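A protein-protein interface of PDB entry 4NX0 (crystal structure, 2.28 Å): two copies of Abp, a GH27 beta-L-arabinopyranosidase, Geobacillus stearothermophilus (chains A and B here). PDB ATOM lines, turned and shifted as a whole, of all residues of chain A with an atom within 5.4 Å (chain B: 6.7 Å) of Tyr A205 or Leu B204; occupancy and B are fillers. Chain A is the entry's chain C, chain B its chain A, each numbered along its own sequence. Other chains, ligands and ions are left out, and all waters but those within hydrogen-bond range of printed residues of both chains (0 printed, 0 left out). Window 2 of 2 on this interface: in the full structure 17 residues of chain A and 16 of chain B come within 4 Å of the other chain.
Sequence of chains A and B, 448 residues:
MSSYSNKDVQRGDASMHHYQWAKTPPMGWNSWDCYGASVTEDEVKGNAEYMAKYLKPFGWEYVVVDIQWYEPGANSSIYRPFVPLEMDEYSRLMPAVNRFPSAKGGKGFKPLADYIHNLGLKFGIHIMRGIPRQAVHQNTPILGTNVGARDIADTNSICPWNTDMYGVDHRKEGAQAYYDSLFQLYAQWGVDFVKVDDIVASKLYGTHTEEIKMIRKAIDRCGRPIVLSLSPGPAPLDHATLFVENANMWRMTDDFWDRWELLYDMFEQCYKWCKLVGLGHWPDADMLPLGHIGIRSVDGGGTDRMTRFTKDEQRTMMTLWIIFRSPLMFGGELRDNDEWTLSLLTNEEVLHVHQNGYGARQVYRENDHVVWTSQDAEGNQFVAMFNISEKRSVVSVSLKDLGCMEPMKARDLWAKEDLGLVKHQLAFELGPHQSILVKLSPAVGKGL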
ATOM      1  N   ARG A 129      13.670  36.130  20.969  1.00  0.00           N
ATOM      2  CA  ARG A 129      12.407  36.464  21.554  1.00  0.00           C
ATOM      3  C   ARG A 129      12.446  36.471  23.041  1.00  0.00           C
ATOM      4  O   ARG A 129      13.008  35.547  23.673  1.00  0.00           O
ATOM      5  CB  ARG A 129      11.369  35.412  21.143  1.00  0.00           C
ATOM      6  CG  ARG A 129       9.962  35.658  21.738  1.00  0.00           C
ATOM      7  CD  ARG A 129       9.078  34.471  21.465  1.00  0.00           C
ATOM      8  NE  ARG A 129       9.606  33.263  22.160  1.00  0.00           N
ATOM      9  CZ  ARG A 129       9.100  32.735  23.271  1.00  0.00           C
ATOM     10  NH1 ARG A 129       8.060  33.281  23.895  1.00  0.00           N
ATOM     11  NH2 ARG A 129       9.625  31.604  23.755  1.00  0.00           N
ATOM     12  N   ASN A 156       5.480  29.997  31.518  1.00  0.00           N
ATOM     13  CA  ASN A 156       5.583  28.784  30.742  1.00  0.00           C
ATOM     14  C   ASN A 156       5.889  29.098  29.297  1.00  0.00           C
ATOM     15  O   ASN A 156       5.094  28.850  28.415  1.00  0.00           O
ATOM     16  CB  ASN A 156       4.291  27.975  30.857  1.00  0.00           C
ATOM     17  CG  ASN A 156       4.336  26.675  30.078  1.00  0.00           C
ATOM     18  OD1 ASN A 156       3.295  26.180  29.575  1.00  0.00           O
ATOM     19  ND2 ASN A 156       5.487  26.186  29.870  1.00  0.00           N
ATOM     20  N   SER A 157       7.053  29.704  29.045  1.00  0.00           N
ATOM     21  CA  SER A 157       7.466  30.030  27.699  1.00  0.00           C
ATOM     22  C   SER A 157       8.999  30.175  27.650  1.00  0.00           C
ATOM     23  O   SER A 157       9.552  31.057  28.266  1.00  0.00           O
ATOM     24  CB  SER A 157       6.830  31.320  27.216  1.00  0.00           C
ATOM     25  OG  SER A 157       7.037  31.486  25.820  1.00  0.00           O
ATOM     26  N   ILE A 158       9.627  29.195  27.051  1.00  0.00           N
ATOM     27  CA  ILE A 158      11.022  29.157  26.855  1.00  0.00           C
ATOM     28  C   ILE A 158      11.303  28.821  25.407  1.00  0.00           C
ATOM     29  O   ILE A 158      10.397  28.463  24.669  1.00  0.00           O
ATOM     30  CB  ILE A 158      11.708  28.132  27.739  1.00  0.00           C
ATOM     31  CG1 ILE A 158      11.164  26.715  27.489  1.00  0.00           C
ATOM     32  CG2 ILE A 158      11.505  28.470  29.212  1.00  0.00           C
ATOM     33  CD1 ILE A 158      12.049  25.623  28.091  1.00  0.00           C
ATOM     34  N   SER A 202       8.469  26.438  17.038  1.00  0.00           N
ATOM     35  CA  SER A 202       8.964  25.952  18.332  1.00  0.00           C
ATOM     36  C   SER A 202       8.380  24.575  18.557  1.00  0.00           C
ATOM     37  O   SER A 202       7.167  24.420  18.574  1.00  0.00           O
ATOM     38  CB  SER A 202       8.478  26.880  19.452  1.00  0.00           C
ATOM     39  OG  SER A 202       8.718  26.343  20.734  1.00  0.00           O
ATOM     40  N   LYS A 203       9.228  23.602  18.826  1.00  0.00           N
ATOM     41  CA  LYS A 203       8.757  22.276  19.205  1.00  0.00           C
ATOM     42  C   LYS A 203       7.783  22.290  20.397  1.00  0.00           C
ATOM     43  O   LYS A 203       6.936  21.461  20.439  1.00  0.00           O
ATOM     44  CB  LYS A 203       9.914  21.363  19.576  1.00  0.00           C
ATOM     45  CG  LYS A 203      10.301  20.366  18.485  1.00  0.00           C
ATOM     46  CD  LYS A 203      10.833  21.163  17.288  1.00  0.00           C
ATOM     47  CE  LYS A 203      10.518  20.576  15.903  1.00  0.00           C
ATOM     48  NZ  LYS A 203      11.410  19.448  15.521  1.00  0.00           N
ATOM     49  N   LEU A 204       7.951  23.191  21.365  1.00  0.00           N
ATOM     50  CA  LEU A 204       7.124  23.210  22.549  1.00  0.00           C
ATOM     51  C   LEU A 204       5.883  24.012  22.397  1.00  0.00           C
ATOM     52  O   LEU A 204       4.843  23.631  22.930  1.00  0.00           O
ATOM     53  CB  LEU A 204       7.872  23.789  23.747  1.00  0.00           C
ATOM     54  CG  LEU A 204       9.094  23.018  24.193  1.00  0.00           C
ATOM     55  CD1 LEU A 204       9.854  23.772  25.239  1.00  0.00           C
ATOM     56  CD2 LEU A 204       8.739  21.613  24.657  1.00  0.00           C
ATOM     57  N   TYR A 205       5.951  25.119  21.669  1.00  0.00           N
ATOM     58  CA  TYR A 205       4.827  26.086  21.708  1.00  0.00           C
ATOM     59  C   TYR A 205       4.311  26.550  20.355  1.00  0.00           C
ATOM     60  O   TYR A 205       3.306  27.227  20.300  1.00  0.00           O
ATOM     61  CB  TYR A 205       5.268  27.324  22.454  1.00  0.00           C
ATOM     62  CG  TYR A 205       5.746  27.072  23.873  1.00  0.00           C
ATOM     63  CD1 TYR A 205       4.855  26.798  24.906  1.00  0.00           C
ATOM     64  CD2 TYR A 205       7.082  27.091  24.171  1.00  0.00           C
ATOM     65  CE1 TYR A 205       5.329  26.612  26.222  1.00  0.00           C
ATOM     66  CE2 TYR A 205       7.569  26.843  25.442  1.00  0.00           C
ATOM     67  CZ  TYR A 205       6.703  26.570  26.450  1.00  0.00           C
ATOM     68  OH  TYR A 205       7.169  26.403  27.736  1.00  0.00           O
ATOM     69  N   GLY A 206       4.893  26.135  19.234  1.00  0.00           N
ATOM     70  CA  GLY A 206       4.335  26.679  17.952  1.00  0.00           C
ATOM     71  C   GLY A 206       4.745  28.144  17.805  1.00  0.00           C
ATOM     72  O   GLY A 206       5.610  28.647  18.526  1.00  0.00           O
ATOM     73  N   THR A 207       4.069  28.842  16.926  1.00  0.00           N
ATOM     74  CA  THR A 207       4.450  30.185  16.505  1.00  0.00           C
ATOM     75  C   THR A 207       4.067  31.149  17.621  1.00  0.00           C
ATOM     76  O   THR A 207       2.954  31.112  18.113  1.00  0.00           O
ATOM     77  CB  THR A 207       3.719  30.553  15.190  1.00  0.00           C
ATOM     78  OG1 THR A 207       4.139  29.642  14.175  1.00  0.00           O
ATOM     79  CG2 THR A 207       4.072  31.948  14.777  1.00  0.00           C
ATOM     80  N   HIS A 208       4.986  32.032  18.007  1.00  0.00           N
ATOM     81  CA  HIS A 208       4.702  33.042  19.029  1.00  0.00           C
ATOM     82  C   HIS A 208       4.071  34.315  18.470  1.00  0.00           C
ATOM     83  O   HIS A 208       4.749  35.310  18.237  1.00  0.00           O
ATOM     84  CB  HIS A 208       5.960  33.326  19.813  1.00  0.00           C
ATOM     85  CG  HIS A 208       6.477  32.139  20.565  1.00  0.00           C
ATOM     86  ND1 HIS A 208       5.869  31.678  21.689  1.00  0.00           N
ATOM     87  CD2 HIS A 208       7.534  31.316  20.354  1.00  0.00           C
ATOM     88  CE1 HIS A 208       6.507  30.624  22.143  1.00  0.00           C
ATOM     89  NE2 HIS A 208       7.549  30.408  21.375  1.00  0.00           N
ATOM     90  N   ILE B 158      11.516  21.872  31.905  1.00  0.00           N
ATOM     91  CA  ILE B 158      10.885  22.645  32.943  1.00  0.00           C
ATOM     92  C   ILE B 158       9.575  21.984  33.307  1.00  0.00           C
ATOM     93  O   ILE B 158       9.148  21.038  32.634  1.00  0.00           O
ATOM     94  CB  ILE B 158      10.599  24.092  32.527  1.00  0.00           C
ATOM     95  CG1 ILE B 158       9.720  24.142  31.284  1.00  0.00           C
ATOM     96  CG2 ILE B 158      11.898  24.804  32.270  1.00  0.00           C
ATOM     97  CD1 ILE B 158       9.094  25.507  31.052  1.00  0.00           C
ATOM     98  N   CYS B 159       8.982  22.467  34.378  1.00  0.00           N
ATOM     99  CA  CYS B 159       7.647  22.122  34.741  1.00  0.00           C
ATOM    100  C   CYS B 159       6.776  23.255  34.164  1.00  0.00           C
ATOM    101  O   CYS B 159       7.047  24.387  34.399  1.00  0.00           O
ATOM    102  CB  CYS B 159       7.495  22.112  36.269  1.00  0.00           C
ATOM    103  SG  CYS B 159       5.805  21.823  36.773  1.00  0.00           S
ATOM    104  N   PRO B 160       5.724  22.921  33.449  1.00  0.00           N
ATOM    105  CA  PRO B 160       4.892  23.956  32.898  1.00  0.00           C
ATOM    106  C   PRO B 160       4.062  24.747  33.888  1.00  0.00           C
ATOM    107  O   PRO B 160       3.527  25.759  33.478  1.00  0.00           O
ATOM    108  CB  PRO B 160       3.929  23.232  31.979  1.00  0.00           C
ATOM    109  CG  PRO B 160       4.256  21.821  32.003  1.00  0.00           C
ATOM    110  CD  PRO B 160       5.379  21.573  32.984  1.00  0.00           C
ATOM    111  N   ALA B 201       3.492  12.924  34.377  1.00  0.00           N
ATOM    112  CA  ALA B 201       2.884  13.505  33.203  1.00  0.00           C
ATOM    113  C   ALA B 201       3.246  14.962  33.157  1.00  0.00           C
ATOM    114  O   ALA B 201       3.484  15.585  34.195  1.00  0.00           O
ATOM    115  CB  ALA B 201       1.383  13.438  33.282  1.00  0.00           C
ATOM    116  N   SER B 202       3.275  15.495  31.956  1.00  0.00           N
ATOM    117  CA  SER B 202       3.677  16.874  31.684  1.00  0.00           C
ATOM    118  C   SER B 202       3.123  17.227  30.343  1.00  0.00           C
ATOM    119  O   SER B 202       3.424  16.540  29.355  1.00  0.00           O
ATOM    120  CB  SER B 202       5.210  16.937  31.613  1.00  0.00           C
ATOM    121  OG  SER B 202       5.657  18.196  31.122  1.00  0.00           O
ATOM    122  N   LYS B 203       2.408  18.314  30.259  1.00  0.00           N
ATOM    123  CA  LYS B 203       1.933  18.825  28.953  1.00  0.00           C
ATOM    124  C   LYS B 203       3.048  19.031  27.965  1.00  0.00           C
ATOM    125  O   LYS B 203       2.838  18.844  26.800  1.00  0.00           O
ATOM    126  CB  LYS B 203       1.214  20.158  29.087  1.00  0.00           C
ATOM    127  CG  LYS B 203      -0.289  20.046  29.025  1.00  0.00           C
ATOM    128  CD  LYS B 203      -0.762  19.226  30.237  1.00  0.00           C
ATOM    129  CE  LYS B 203      -1.984  18.316  29.993  1.00  0.00           C
ATOM    130  NZ  LYS B 203      -3.287  19.047  30.006  1.00  0.00           N
ATOM    131  N   LEU B 204       4.246  19.413  28.412  1.00  0.00           N
ATOM    132  CA  LEU B 204       5.331  19.685  27.456  1.00  0.00           C
ATOM    133  C   LEU B 204       6.135  18.499  27.106  1.00  0.00           C
ATOM    134  O   LEU B 204       6.644  18.394  25.985  1.00  0.00           O
ATOM    135  CB  LEU B 204       6.306  20.704  28.049  1.00  0.00           C
ATOM    136  CG  LEU B 204       5.723  22.098  28.328  1.00  0.00           C
ATOM    137  CD1 LEU B 204       6.717  22.952  29.085  1.00  0.00           C
ATOM    138  CD2 LEU B 204       5.276  22.769  27.039  1.00  0.00           C
ATOM    139  N   TYR B 205       6.339  17.595  28.048  1.00  0.00           N
ATOM    140  CA  TYR B 205       7.360  16.571  27.855  1.00  0.00           C
ATOM    141  C   TYR B 205       6.901  15.127  28.079  1.00  0.00           C
ATOM    142  O   TYR B 205       7.679  14.226  27.855  1.00  0.00           O
ATOM    143  CB  TYR B 205       8.495  16.813  28.815  1.00  0.00           C
ATOM    144  CG  TYR B 205       9.153  18.116  28.634  1.00  0.00           C
ATOM    145  CD1 TYR B 205      10.012  18.356  27.530  1.00  0.00           C
ATOM    146  CD2 TYR B 205       8.976  19.125  29.533  1.00  0.00           C
ATOM    147  CE1 TYR B 205      10.648  19.600  27.420  1.00  0.00           C
ATOM    148  CE2 TYR B 205       9.585  20.401  29.363  1.00  0.00           C
ATOM    149  CZ  TYR B 205      10.399  20.627  28.338  1.00  0.00           C
ATOM    150  OH  TYR B 205      11.027  21.866  28.224  1.00  0.00           O
ATOM    151  N   GLY B 206       5.705  14.879  28.568  1.00  0.00           N
ATOM    152  CA  GLY B 206       5.444  13.461  28.908  1.00  0.00           C
ATOM    153  C   GLY B 206       6.235  13.006  30.174  1.00  0.00           C
ATOM    154  O   GLY B 206       6.719  13.843  30.940  1.00  0.00           O
ATOM    155  N   HIS B 208       8.835  11.741  32.768  1.00  0.00           N
ATOM    156  CA  HIS B 208      10.299  11.875  32.944  1.00  0.00           C
ATOM    157  C   HIS B 208      10.901  10.600  33.447  1.00  0.00           C
ATOM    158  O   HIS B 208      11.194  10.429  34.647  1.00  0.00           O
ATOM    159  CB  HIS B 208      10.550  13.066  33.837  1.00  0.00           C
ATOM    160  CG  HIS B 208      10.197  14.360  33.165  1.00  0.00           C
ATOM    161  ND1 HIS B 208       9.106  15.161  33.480  1.00  0.00           N
ATOM    162  CD2 HIS B 208      10.802  14.953  32.132  1.00  0.00           C
ATOM    163  CE1 HIS B 208       9.092  16.224  32.686  1.00  0.00           C
ATOM    164  NE2 HIS B 208      10.114  16.101  31.854  1.00  0.00           N
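The backbone NH (N) of Tyr B205 sits at hydrogen-bond distance from the side-chain hydroxyl (OG) of Ser B202 (3.2 Å).
The side-chain amide nitrogen of Asn A156 is in hydrogen-bond range of the side-chain hydroxyl of Tyr A205 (2.7 Å).
OG of Ser A202 lies within hydrogen-bond range of N of Tyr A205 (3.2 Å).
The side-chain hydroxyl (OG) of Ser B202 lies close to the backbone NH (N) of Leu B204, 3.3 Å away.
NH2 of Arg A129 is in hydrogen-bond range of O of Ile A158 (3.4 Å).
The backbone NH (N) of Leu A204 lies close to the side-chain hydroxyl (OG) of Ser A202, at 3.3 Å.
Among the printed residues, pairs that only touch across the chains: Asn A156 with Pro B160, Asn A156 with Leu B204, Leu A204 with Tyr B205, Tyr A205 with Leu B204, Asn A156 with Ile B158, Ile A158 with Tyr B205 and Tyr A205 with Ile B158.
Tyr A205 touches just these residues of chain B: Ile B158 and Leu B204.
Printed residues of chain A within 4 Å of Tyr B205: Ile A158 (3.9 Å) and Leu A204 (3.7 Å).
Of the printed residues of chain B, Ile A158 touches Tyr B205 (3.9 Å).
Printed residues of chain B within 4 Å of Asn A156: Ile B158 (3.9 Å), Pro B160 (3.5 Å) and Leu B204 (3.5 Å).
The nearest printed residue of chain B that does not touch Ile A158 is Ile B158 (4.2 Å).
Printed residues of chain A that touch a printed residue of chain B: Asn A156, Ile A158, Leu A204 and Tyr A205.
Of the 10 printed residues of chain B, 4 touch a printed residue of chain A.
Hydrophobic or aromatic side chains of chain B within 4 Å of the printed part of chain A: Ile B158, Pro B160, Leu B204 and Tyr B205.
Ile A158 touches Tyr B205, and with the chains exchanged Tyr A205 touches Ile B158.
Leu A204 touches Tyr B205, and with the chains exchanged Tyr A205 touches Leu B204.
Of the 7 pairs that touch across the chains among the printed residues, 4 have their exchanged pair printed and touching as well.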
